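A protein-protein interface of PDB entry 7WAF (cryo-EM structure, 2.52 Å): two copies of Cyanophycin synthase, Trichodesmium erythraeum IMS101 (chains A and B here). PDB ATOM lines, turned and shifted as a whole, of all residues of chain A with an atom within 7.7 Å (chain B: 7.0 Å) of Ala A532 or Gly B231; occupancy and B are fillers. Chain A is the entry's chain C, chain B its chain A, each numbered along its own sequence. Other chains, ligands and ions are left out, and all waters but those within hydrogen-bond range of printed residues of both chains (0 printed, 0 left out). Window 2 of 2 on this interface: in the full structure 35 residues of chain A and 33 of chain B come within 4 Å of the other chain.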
ATOM      1  N   TYR A 519      10.045 -10.013 -33.799  1.00  0.00           N
ATOM      2  CA  TYR A 519       9.231  -8.816 -33.919  1.00  0.00           C
ATOM      3  C   TYR A 519       8.768  -8.343 -32.553  1.00  0.00           C
ATOM      4  O   TYR A 519       8.396  -9.146 -31.691  1.00  0.00           O
ATOM      5  CB  TYR A 519       8.024  -9.039 -34.843  1.00  0.00           C
ATOM      6  CG  TYR A 519       7.012 -10.052 -34.370  1.00  0.00           C
ATOM      7  CD1 TYR A 519       7.238 -11.412 -34.520  1.00  0.00           C
ATOM      8  CD2 TYR A 519       5.814  -9.647 -33.801  1.00  0.00           C
ATOM      9  CE1 TYR A 519       6.307 -12.338 -34.104  1.00  0.00           C
ATOM     10  CE2 TYR A 519       4.879 -10.565 -33.379  1.00  0.00           C
ATOM     11  CZ  TYR A 519       5.131 -11.909 -33.532  1.00  0.00           C
ATOM     12  OH  TYR A 519       4.199 -12.829 -33.112  1.00  0.00           O
ATOM     13  N   GLY A 524       3.979  -7.603 -26.888  1.00  0.00           N
ATOM     14  CA  GLY A 524       5.220  -8.126 -26.358  1.00  0.00           C
ATOM     15  C   GLY A 524       6.189  -8.449 -27.471  1.00  0.00           C
ATOM     16  O   GLY A 524       5.880  -8.329 -28.660  1.00  0.00           O
ATOM     17  N   THR A 525       7.378  -8.875 -27.055  1.00  0.00           N
ATOM     18  CA  THR A 525       8.466  -9.204 -27.967  1.00  0.00           C
ATOM     19  C   THR A 525       8.451 -10.703 -28.233  1.00  0.00           C
ATOM     20  O   THR A 525       8.540 -11.501 -27.293  1.00  0.00           O
ATOM     21  CB  THR A 525       9.810  -8.780 -27.376  1.00  0.00           C
ATOM     22  OG1 THR A 525       9.877  -7.351 -27.313  1.00  0.00           O
ATOM     23  CG2 THR A 525      10.952  -9.301 -28.222  1.00  0.00           C
ATOM     24  N   TYR A 526       8.352 -11.080 -29.508  1.00  0.00           N
ATOM     25  CA  TYR A 526       8.304 -12.472 -29.925  1.00  0.00           C
ATOM     26  C   TYR A 526       9.495 -12.785 -30.817  1.00  0.00           C
ATOM     27  O   TYR A 526       9.942 -11.936 -31.596  1.00  0.00           O
ATOM     28  CB  TYR A 526       7.013 -12.791 -30.687  1.00  0.00           C
ATOM     29  CG  TYR A 526       5.751 -12.707 -29.866  1.00  0.00           C
ATOM     30  CD1 TYR A 526       5.161 -11.483 -29.588  1.00  0.00           C
ATOM     31  CD2 TYR A 526       5.141 -13.854 -29.379  1.00  0.00           C
ATOM     32  CE1 TYR A 526       4.006 -11.403 -28.842  1.00  0.00           C
ATOM     33  CE2 TYR A 526       3.986 -13.784 -28.631  1.00  0.00           C
ATOM     34  CZ  TYR A 526       3.421 -12.556 -28.367  1.00  0.00           C
ATOM     35  OH  TYR A 526       2.268 -12.480 -27.621  1.00  0.00           O
ATOM     36  N   ILE A 527      10.003 -14.006 -30.694  1.00  0.00           N
ATOM     37  CA  ILE A 527      11.038 -14.533 -31.573  1.00  0.00           C
ATOM     38  C   ILE A 527      10.499 -15.836 -32.143  1.00  0.00           C
ATOM     39  O   ILE A 527      10.346 -16.823 -31.413  1.00  0.00           O
ATOM     40  CB  ILE A 527      12.365 -14.753 -30.838  1.00  0.00           C
ATOM     41  CG1 ILE A 527      12.887 -13.425 -30.289  1.00  0.00           C
ATOM     42  CG2 ILE A 527      13.383 -15.387 -31.766  1.00  0.00           C
ATOM     43  CD1 ILE A 527      14.225 -13.532 -29.614  1.00  0.00           C
ATOM     44  N   GLY A 528      10.218 -15.845 -33.440  1.00  0.00           N
ATOM     45  CA  GLY A 528       9.562 -16.986 -34.044  1.00  0.00           C
ATOM     46  C   GLY A 528       8.158 -17.180 -33.510  1.00  0.00           C
ATOM     47  O   GLY A 528       7.342 -16.255 -33.542  1.00  0.00           O
ATOM     48  N   GLU A 529       7.865 -18.377 -33.010  1.00  0.00           N
ATOM     49  CA  GLU A 529       6.543 -18.708 -32.497  1.00  0.00           C
ATOM     50  C   GLU A 529       6.426 -18.560 -30.987  1.00  0.00           C
ATOM     51  O   GLU A 529       5.359 -18.840 -30.435  1.00  0.00           O
ATOM     52  CB  GLU A 529       6.167 -20.138 -32.897  1.00  0.00           C
ATOM     53  CG  GLU A 529       6.154 -20.384 -34.395  1.00  0.00           C
ATOM     54  CD  GLU A 529       5.007 -19.675 -35.091  1.00  0.00           C
ATOM     55  OE1 GLU A 529       3.974 -19.429 -34.434  1.00  0.00           O
ATOM     56  OE2 GLU A 529       5.141 -19.365 -36.293  1.00  0.00           O
ATOM     57  N   TYR A 530       7.482 -18.128 -30.306  1.00  0.00           N
ATOM     58  CA  TYR A 530       7.501 -18.089 -28.852  1.00  0.00           C
ATOM     59  C   TYR A 530       7.694 -16.664 -28.357  1.00  0.00           C
ATOM     60  O   TYR A 530       8.345 -15.841 -29.005  1.00  0.00           O
ATOM     61  CB  TYR A 530       8.604 -18.991 -28.294  1.00  0.00           C
ATOM     62  CG  TYR A 530       8.456 -20.437 -28.698  1.00  0.00           C
ATOM     63  CD1 TYR A 530       7.468 -21.235 -28.141  1.00  0.00           C
ATOM     64  CD2 TYR A 530       9.297 -21.002 -29.646  1.00  0.00           C
ATOM     65  CE1 TYR A 530       7.327 -22.556 -28.510  1.00  0.00           C
ATOM     66  CE2 TYR A 530       9.163 -22.320 -30.021  1.00  0.00           C
ATOM     67  CZ  TYR A 530       8.177 -23.093 -29.449  1.00  0.00           C
ATOM     68  OH  TYR A 530       8.040 -24.410 -29.822  1.00  0.00           O
ATOM     69  N   LEU A 531       7.120 -16.385 -27.190  1.00  0.00           N
ATOM     70  CA  LEU A 531       7.149 -15.050 -26.604  1.00  0.00           C
ATOM     71  C   LEU A 531       8.468 -14.849 -25.869  1.00  0.00           C
ATOM     72  O   LEU A 531       8.729 -15.503 -24.854  1.00  0.00           O
ATOM     73  CB  LEU A 531       5.962 -14.865 -25.666  1.00  0.00           C
ATOM     74  CG  LEU A 531       5.961 -13.617 -24.788  1.00  0.00           C
ATOM     75  CD1 LEU A 531       5.392 -12.431 -25.540  1.00  0.00           C
ATOM     76  CD2 LEU A 531       5.163 -13.886 -23.531  1.00  0.00           C
ATOM     77  N   ALA A 532       9.303 -13.946 -26.383  1.00  0.00           N
ATOM     78  CA  ALA A 532      10.578 -13.658 -25.737  1.00  0.00           C
ATOM     79  C   ALA A 532      10.417 -12.775 -24.507  1.00  0.00           C
ATOM     80  O   ALA A 532      11.150 -12.949 -23.528  1.00  0.00           O
ATOM     81  CB  ALA A 532      11.536 -13.001 -26.729  1.00  0.00           C
ATOM     82  N   GLU A 533       9.480 -11.829 -24.530  1.00  0.00           N
ATOM     83  CA  GLU A 533       9.332 -10.912 -23.407  1.00  0.00           C
ATOM     84  C   GLU A 533       7.918 -10.349 -23.380  1.00  0.00           C
ATOM     85  O   GLU A 533       7.326 -10.095 -24.431  1.00  0.00           O
ATOM     86  CB  GLU A 533      10.351  -9.770 -23.489  1.00  0.00           C
ATOM     87  CG  GLU A 533      10.310  -8.817 -22.306  1.00  0.00           C
ATOM     88  CD  GLU A 533      11.360  -7.728 -22.392  1.00  0.00           C
ATOM     89  OE1 GLU A 533      12.110  -7.701 -23.389  1.00  0.00           O
ATOM     90  OE2 GLU A 533      11.433  -6.898 -21.463  1.00  0.00           O
ATOM     91  N   THR A 534       7.396 -10.141 -22.174  1.00  0.00           N
ATOM     92  CA  THR A 534       6.092  -9.530 -21.975  1.00  0.00           C
ATOM     93  C   THR A 534       6.223  -8.015 -21.849  1.00  0.00           C
ATOM     94  O   THR A 534       7.318  -7.451 -21.893  1.00  0.00           O
ATOM     95  CB  THR A 534       5.417 -10.094 -20.724  1.00  0.00           C
ATOM     96  OG1 THR A 534       6.193  -9.753 -19.569  1.00  0.00           O
ATOM     97  CG2 THR A 534       5.304 -11.602 -20.812  1.00  0.00           C
ATOM     98  N   ASN A 537       7.072  -3.093 -24.625  1.00  0.00           N
ATOM     99  CA  ASN A 537       8.136  -3.515 -25.538  1.00  0.00           C
ATOM    100  C   ASN A 537       7.987  -2.870 -26.918  1.00  0.00           C
ATOM    101  O   ASN A 537       7.772  -3.538 -27.930  1.00  0.00           O
ATOM    102  CB  ASN A 537       8.179  -5.041 -25.652  1.00  0.00           C
ATOM    103  CG  ASN A 537       8.667  -5.702 -24.385  1.00  0.00           C
ATOM    104  OD1 ASN A 537       9.612  -5.236 -23.752  1.00  0.00           O
ATOM    105  ND2 ASN A 537       8.030  -6.802 -24.012  1.00  0.00           N
ATOM    106  N   LEU A 545      16.891  -6.384 -27.906  1.00  0.00           N
ATOM    107  CA  LEU A 545      16.681  -7.807 -27.659  1.00  0.00           C
ATOM    108  C   LEU A 545      16.526  -8.574 -28.964  1.00  0.00           C
ATOM    109  O   LEU A 545      17.063  -9.677 -29.114  1.00  0.00           O
ATOM    110  CB  LEU A 545      15.455  -8.005 -26.768  1.00  0.00           C
ATOM    111  CG  LEU A 545      15.244  -9.376 -26.121  1.00  0.00           C
ATOM    112  CD1 LEU A 545      14.557  -9.216 -24.783  1.00  0.00           C
ATOM    113  CD2 LEU A 545      14.432 -10.296 -27.016  1.00  0.00           C
ATOM    114  N   ILE A 546      15.786  -8.010 -29.920  1.00  0.00           N
ATOM    115  CA  ILE A 546      15.614  -8.665 -31.211  1.00  0.00           C
ATOM    116  C   ILE A 546      16.924  -8.664 -31.989  1.00  0.00           C
ATOM    117  O   ILE A 546      17.341  -9.688 -32.539  1.00  0.00           O
ATOM    118  CB  ILE A 546      14.485  -7.990 -32.008  1.00  0.00           C
ATOM    119  CG1 ILE A 546      13.131  -8.287 -31.367  1.00  0.00           C
ATOM    120  CG2 ILE A 546      14.496  -8.461 -33.448  1.00  0.00           C
ATOM    121  CD1 ILE A 546      12.851  -9.758 -31.225  1.00  0.00           C
ATOM    122  N   ASP A 549      19.670 -11.178 -30.751  1.00  0.00           N
ATOM    123  CA  ASP A 549      19.377 -12.604 -30.669  1.00  0.00           C
ATOM    124  C   ASP A 549      20.103 -13.351 -31.782  1.00  0.00           C
ATOM    125  O   ASP A 549      19.960 -12.995 -32.954  1.00  0.00           O
ATOM    126  CB  ASP A 549      17.879 -12.856 -30.764  1.00  0.00           C
ATOM    127  CG  ASP A 549      17.509 -14.283 -30.410  1.00  0.00           C
ATOM    128  OD1 ASP A 549      17.332 -14.572 -29.209  1.00  0.00           O
ATOM    129  OD2 ASP A 549      17.397 -15.116 -31.333  1.00  0.00           O
ATOM    130  N   ILE B 226      23.658 -10.820 -19.094  1.00  0.00           N
ATOM    131  CA  ILE B 226      23.430 -11.099 -20.509  1.00  0.00           C
ATOM    132  C   ILE B 226      22.094 -11.801 -20.708  1.00  0.00           C
ATOM    133  O   ILE B 226      21.324 -11.453 -21.612  1.00  0.00           O
ATOM    134  CB  ILE B 226      24.593 -11.926 -21.087  1.00  0.00           C
ATOM    135  CG1 ILE B 226      25.839 -11.059 -21.222  1.00  0.00           C
ATOM    136  CG2 ILE B 226      24.222 -12.498 -22.436  1.00  0.00           C
ATOM    137  CD1 ILE B 226      25.639  -9.840 -22.086  1.00  0.00           C
ATOM    138  N   LEU B 227      21.792 -12.792 -19.868  1.00  0.00           N
ATOM    139  CA  LEU B 227      20.544 -13.530 -20.029  1.00  0.00           C
ATOM    140  C   LEU B 227      19.337 -12.658 -19.708  1.00  0.00           C
ATOM    141  O   LEU B 227      18.287 -12.787 -20.346  1.00  0.00           O
ATOM    142  CB  LEU B 227      20.561 -14.779 -19.151  1.00  0.00           C
ATOM    143  CG  LEU B 227      21.544 -15.870 -19.577  1.00  0.00           C
ATOM    144  CD1 LEU B 227      21.396 -17.098 -18.699  1.00  0.00           C
ATOM    145  CD2 LEU B 227      21.342 -16.225 -21.039  1.00  0.00           C
ATOM    146  N   LYS B 228      19.463 -11.766 -18.722  1.00  0.00           N
ATOM    147  CA  LYS B 228      18.371 -10.850 -18.416  1.00  0.00           C
ATOM    148  C   LYS B 228      18.139  -9.871 -19.558  1.00  0.00           C
ATOM    149  O   LYS B 228      16.991  -9.537 -19.872  1.00  0.00           O
ATOM    150  CB  LYS B 228      18.662 -10.107 -17.114  1.00  0.00           C
ATOM    151  CG  LYS B 228      17.543  -9.187 -16.665  1.00  0.00           C
ATOM    152  CD  LYS B 228      17.810  -8.629 -15.279  1.00  0.00           C
ATOM    153  CE  LYS B 228      16.815  -7.537 -14.928  1.00  0.00           C
ATOM    154  NZ  LYS B 228      15.422  -8.058 -14.870  1.00  0.00           N
ATOM    155  N   ASP B 229      19.216  -9.396 -20.189  1.00  0.00           N
ATOM    156  CA  ASP B 229      19.064  -8.525 -21.348  1.00  0.00           C
ATOM    157  C   ASP B 229      18.388  -9.231 -22.515  1.00  0.00           C
ATOM    158  O   ASP B 229      17.813  -8.562 -23.381  1.00  0.00           O
ATOM    159  CB  ASP B 229      20.426  -7.986 -21.788  1.00  0.00           C
ATOM    160  CG  ASP B 229      20.974  -6.941 -20.838  1.00  0.00           C
ATOM    161  OD1 ASP B 229      20.185  -6.387 -20.044  1.00  0.00           O
ATOM    162  OD2 ASP B 229      22.192  -6.672 -20.884  1.00  0.00           O
ATOM    163  N   ALA B 230      18.441 -10.560 -22.561  1.00  0.00           N
ATOM    164  CA  ALA B 230      17.816 -11.337 -23.620  1.00  0.00           C
ATOM    165  C   ALA B 230      16.422 -11.830 -23.254  1.00  0.00           C
ATOM    166  O   ALA B 230      15.820 -12.574 -24.032  1.00  0.00           O
ATOM    167  CB  ALA B 230      18.700 -12.529 -23.992  1.00  0.00           C
ATOM    168  N   GLY B 231      15.900 -11.442 -22.094  1.00  0.00           N
ATOM    169  CA  GLY B 231      14.586 -11.878 -21.672  1.00  0.00           C
ATOM    170  C   GLY B 231      14.538 -13.236 -21.011  1.00  0.00           C
ATOM    171  O   GLY B 231      13.442 -13.714 -20.700  1.00  0.00           O
ATOM    172  N   VAL B 232      15.681 -13.869 -20.791  1.00  0.00           N
ATOM    173  CA  VAL B 232      15.703 -15.181 -20.131  1.00  0.00           C
ATOM    174  C   VAL B 232      15.380 -15.006 -18.655  1.00  0.00           C
ATOM    175  O   VAL B 232      15.926 -14.092 -18.009  1.00  0.00           O
ATOM    176  CB  VAL B 232      17.067 -15.846 -20.328  1.00  0.00           C
ATOM    177  CG1 VAL B 232      17.127 -17.174 -19.602  1.00  0.00           C
ATOM    178  CG2 VAL B 232      17.351 -16.032 -21.808  1.00  0.00           C
ATOM    179  N   PRO B 233      14.510 -15.834 -18.072  1.00  0.00           N
ATOM    180  CA  PRO B 233      14.143 -15.654 -16.661  1.00  0.00           C
ATOM    181  C   PRO B 233      15.224 -16.092 -15.685  1.00  0.00           C
ATOM    182  O   PRO B 233      15.214 -17.231 -15.214  1.00  0.00           O
ATOM    183  CB  PRO B 233      12.885 -16.521 -16.516  1.00  0.00           C
ATOM    184  CG  PRO B 233      13.029 -17.557 -17.572  1.00  0.00           C
ATOM    185  CD  PRO B 233      13.686 -16.864 -18.727  1.00  0.00           C
ATOM    186  N   VAL B 234      16.169 -15.207 -15.387  1.00  0.00           N
ATOM    187  CA  VAL B 234      17.206 -15.478 -14.392  1.00  0.00           C
ATOM    188  C   VAL B 234      16.696 -15.078 -13.012  1.00  0.00           C
ATOM    189  O   VAL B 234      15.767 -14.264 -12.912  1.00  0.00           O
ATOM    190  CB  VAL B 234      18.509 -14.743 -14.739  1.00  0.00           C
ATOM    191  CG1 VAL B 234      19.144 -15.362 -15.964  1.00  0.00           C
ATOM    192  CG2 VAL B 234      18.240 -13.266 -14.962  1.00  0.00           C
ATOM    193  N   GLU B 411       8.705 -25.374 -25.663  1.00  0.00           N
ATOM    194  CA  GLU B 411       9.094 -23.994 -25.401  1.00  0.00           C
ATOM    195  C   GLU B 411      10.348 -23.937 -24.541  1.00  0.00           C
ATOM    196  O   GLU B 411      11.226 -23.095 -24.760  1.00  0.00           O
ATOM    197  CB  GLU B 411       7.944 -23.245 -24.729  1.00  0.00           C
ATOM    198  CG  GLU B 411       8.219 -21.775 -24.479  1.00  0.00           C
ATOM    199  CD  GLU B 411       6.949 -20.961 -24.350  1.00  0.00           C
ATOM    200  OE1 GLU B 411       5.871 -21.478 -24.712  1.00  0.00           O
ATOM    201  OE2 GLU B 411       7.025 -19.806 -23.883  1.00  0.00           O
ATOM    202  N   TRP B 414      13.312 -24.705 -26.780  1.00  0.00           N
ATOM    203  CA  TRP B 414      13.672 -23.517 -27.547  1.00  0.00           C
ATOM    204  C   TRP B 414      14.413 -22.503 -26.684  1.00  0.00           C
ATOM    205  O   TRP B 414      15.434 -21.945 -27.104  1.00  0.00           O
ATOM    206  CB  TRP B 414      12.410 -22.904 -28.154  1.00  0.00           C
ATOM    207  CG  TRP B 414      12.548 -21.491 -28.620  1.00  0.00           C
ATOM    208  CD1 TRP B 414      13.000 -21.068 -29.834  1.00  0.00           C
ATOM    209  CD2 TRP B 414      12.202 -20.311 -27.887  1.00  0.00           C
ATOM    210  NE1 TRP B 414      12.968 -19.697 -29.899  1.00  0.00           N
ATOM    211  CE2 TRP B 414      12.481 -19.208 -28.715  1.00  0.00           C
ATOM    212  CE3 TRP B 414      11.690 -20.081 -26.609  1.00  0.00           C
ATOM    213  CZ2 TRP B 414      12.260 -17.896 -28.308  1.00  0.00           C
ATOM    214  CZ3 TRP B 414      11.477 -18.778 -26.205  1.00  0.00           C
ATOM    215  CH2 TRP B 414      11.763 -17.702 -27.050  1.00  0.00           C
ATOM    216  N   LEU B 415      13.923 -22.270 -25.465  1.00  0.00           N
ATOM    217  CA  LEU B 415      14.561 -21.304 -24.577  1.00  0.00           C
ATOM    218  C   LEU B 415      15.977 -21.732 -24.209  1.00  0.00           C
ATOM    219  O   LEU B 415      16.892 -20.903 -24.171  1.00  0.00           O
ATOM    220  CB  LEU B 415      13.717 -21.115 -23.318  1.00  0.00           C
ATOM    221  CG  LEU B 415      14.284 -20.163 -22.267  1.00  0.00           C
ATOM    222  CD1 LEU B 415      14.318 -18.743 -22.798  1.00  0.00           C
ATOM    223  CD2 LEU B 415      13.472 -20.240 -20.988  1.00  0.00           C
ATOM    224  N   ARG B 418      18.300 -21.279 -27.085  1.00  0.00           N
ATOM    225  CA  ARG B 418      18.636 -19.861 -27.169  1.00  0.00           C
ATOM    226  C   ARG B 418      19.661 -19.468 -26.118  1.00  0.00           C
ATOM    227  O   ARG B 418      20.554 -18.665 -26.392  1.00  0.00           O
ATOM    228  CB  ARG B 418      17.387 -18.999 -27.021  1.00  0.00           C
ATOM    229  CG  ARG B 418      16.667 -18.726 -28.314  1.00  0.00           C
ATOM    230  CD  ARG B 418      15.583 -17.698 -28.092  1.00  0.00           C
ATOM    231  NE  ARG B 418      16.128 -16.382 -27.784  1.00  0.00           N
ATOM    232  CZ  ARG B 418      15.846 -15.693 -26.686  1.00  0.00           C
ATOM    233  NH1 ARG B 418      15.039 -16.174 -25.756  1.00  0.00           N
ATOM    234  NH2 ARG B 418      16.388 -14.490 -26.519  1.00  0.00           N
ATOM    235  N   ILE B 422      23.194 -17.852 -26.953  1.00  0.00           N
ATOM    236  CA  ILE B 422      23.466 -16.505 -26.463  1.00  0.00           C
ATOM    237  C   ILE B 422      24.780 -16.470 -25.697  1.00  0.00           C
ATOM    238  O   ILE B 422      25.597 -15.559 -25.885  1.00  0.00           O
ATOM    239  CB  ILE B 422      22.292 -16.011 -25.598  1.00  0.00           C
ATOM    240  CG1 ILE B 422      21.139 -15.534 -26.481  1.00  0.00           C
ATOM    241  CG2 ILE B 422      22.736 -14.898 -24.673  1.00  0.00           C
ATOM    242  CD1 ILE B 422      19.804 -15.531 -25.779  1.00  0.00           C
ATOM    243  N   ARG B 442       7.656 -19.748 -17.832  1.00  0.00           N
ATOM    244  CA  ARG B 442       6.903 -18.549 -17.490  1.00  0.00           C
ATOM    245  C   ARG B 442       5.686 -18.859 -16.628  1.00  0.00           C
ATOM    246  O   ARG B 442       5.380 -18.105 -15.699  1.00  0.00           O
ATOM    247  CB  ARG B 442       6.463 -17.819 -18.759  1.00  0.00           C
ATOM    248  CG  ARG B 442       7.605 -17.319 -19.622  1.00  0.00           C
ATOM    249  CD  ARG B 442       7.091 -16.757 -20.939  1.00  0.00           C
ATOM    250  NE  ARG B 442       6.481 -17.786 -21.772  1.00  0.00           N
ATOM    251  CZ  ARG B 442       5.173 -17.954 -21.918  1.00  0.00           C
ATOM    252  NH1 ARG B 442       4.303 -17.174 -21.299  1.00  0.00           N
ATOM    253  NH2 ARG B 442       4.729 -18.931 -22.704  1.00  0.00           N
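NE of Arg B418 lies within salt-bridge range of OD1 of Asp A549 (2.6 Å).
O of Thr A525 lies within hydrogen-bond range of N of Ala A532, 2.7 Å away.
NH2 of Arg B418 is in hydrogen-bond range of O of Ala B230, at 3.2 Å.
The guanidinium group of Arg B442 lies within salt-bridge range of the side-chain carboxylate of Glu B411, 2.7 Å away.
Ile A527 touches Trp B414.
Arg B418 touches Ile A527 (NE to CD1, 3.9 Å).
Glu B411 touches Tyr A530.
CD2 of Tyr A530 touches CG of Trp B414 (3.4 Å).
Ala A532 touches Gly B231 (O to O, 3.7 Å).
CD1 of Leu A545 touches O of Asp B229, at 3.6 Å.
CD1 of Leu A545 touches C of Ala B230, 3.6 Å away.
N of Gly B231 touches CD1 of Leu A545, 3.7 Å away.
Printed residues of chain B within 4 Å of Ile A527: Trp B414 (3.8 Å) and Arg B418 (3.9 Å).
Gly A528 touches none of the printed residues of chain B.
Of chain B, only Gly B231 (3.7 Å) comes within 4 Å of Ala A532.
Of the printed residues of chain B, Leu A545 touches Asp B229 (3.6 Å), Ala B230 (3.6 Å) and Gly B231 (3.7 Å).
Ala B230 touches one residue of chain A.
Pro B233 touches none of the printed residues of chain A.
Of the printed residues of chain A, Trp B414 touches Ile A527 (3.8 Å) and Tyr A530 (3.4 Å).
Printed residues of chain A within 4 Å of Arg B418: Ile A527 and Asp A549.
The nearest residue of chain B that does not touch Ala A532 is Trp B414 (4.4 Å).
The nearest residue of chain A that does not touch Gly B231 is Glu A533 (5.1 Å).
The nearest printed residue of chain B that does not touch Asp A549 is Ile B422 (4.3 Å).
Printed residues of chain A that touch a printed residue of chain B: Ile A527, Tyr A530, Ala A532, Leu A545 and Asp A549.
Hydrophobic or aromatic side chains of chain A that line the printed part of chain B: Ile A527, Tyr A530 and Leu A545.
Of the 15 printed residues of chain B, 6 touch a printed residue of chain A.
Hydrophobic or aromatic side chains of chain B that line the printed part of chain A: Trp B414.
Among the printed residues, Asp or Glu carboxylates within 4 Å of a Lys or Arg side-chain nitrogen of the other chain: Asp A549 with Arg B418.
No position is printed for both chains.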
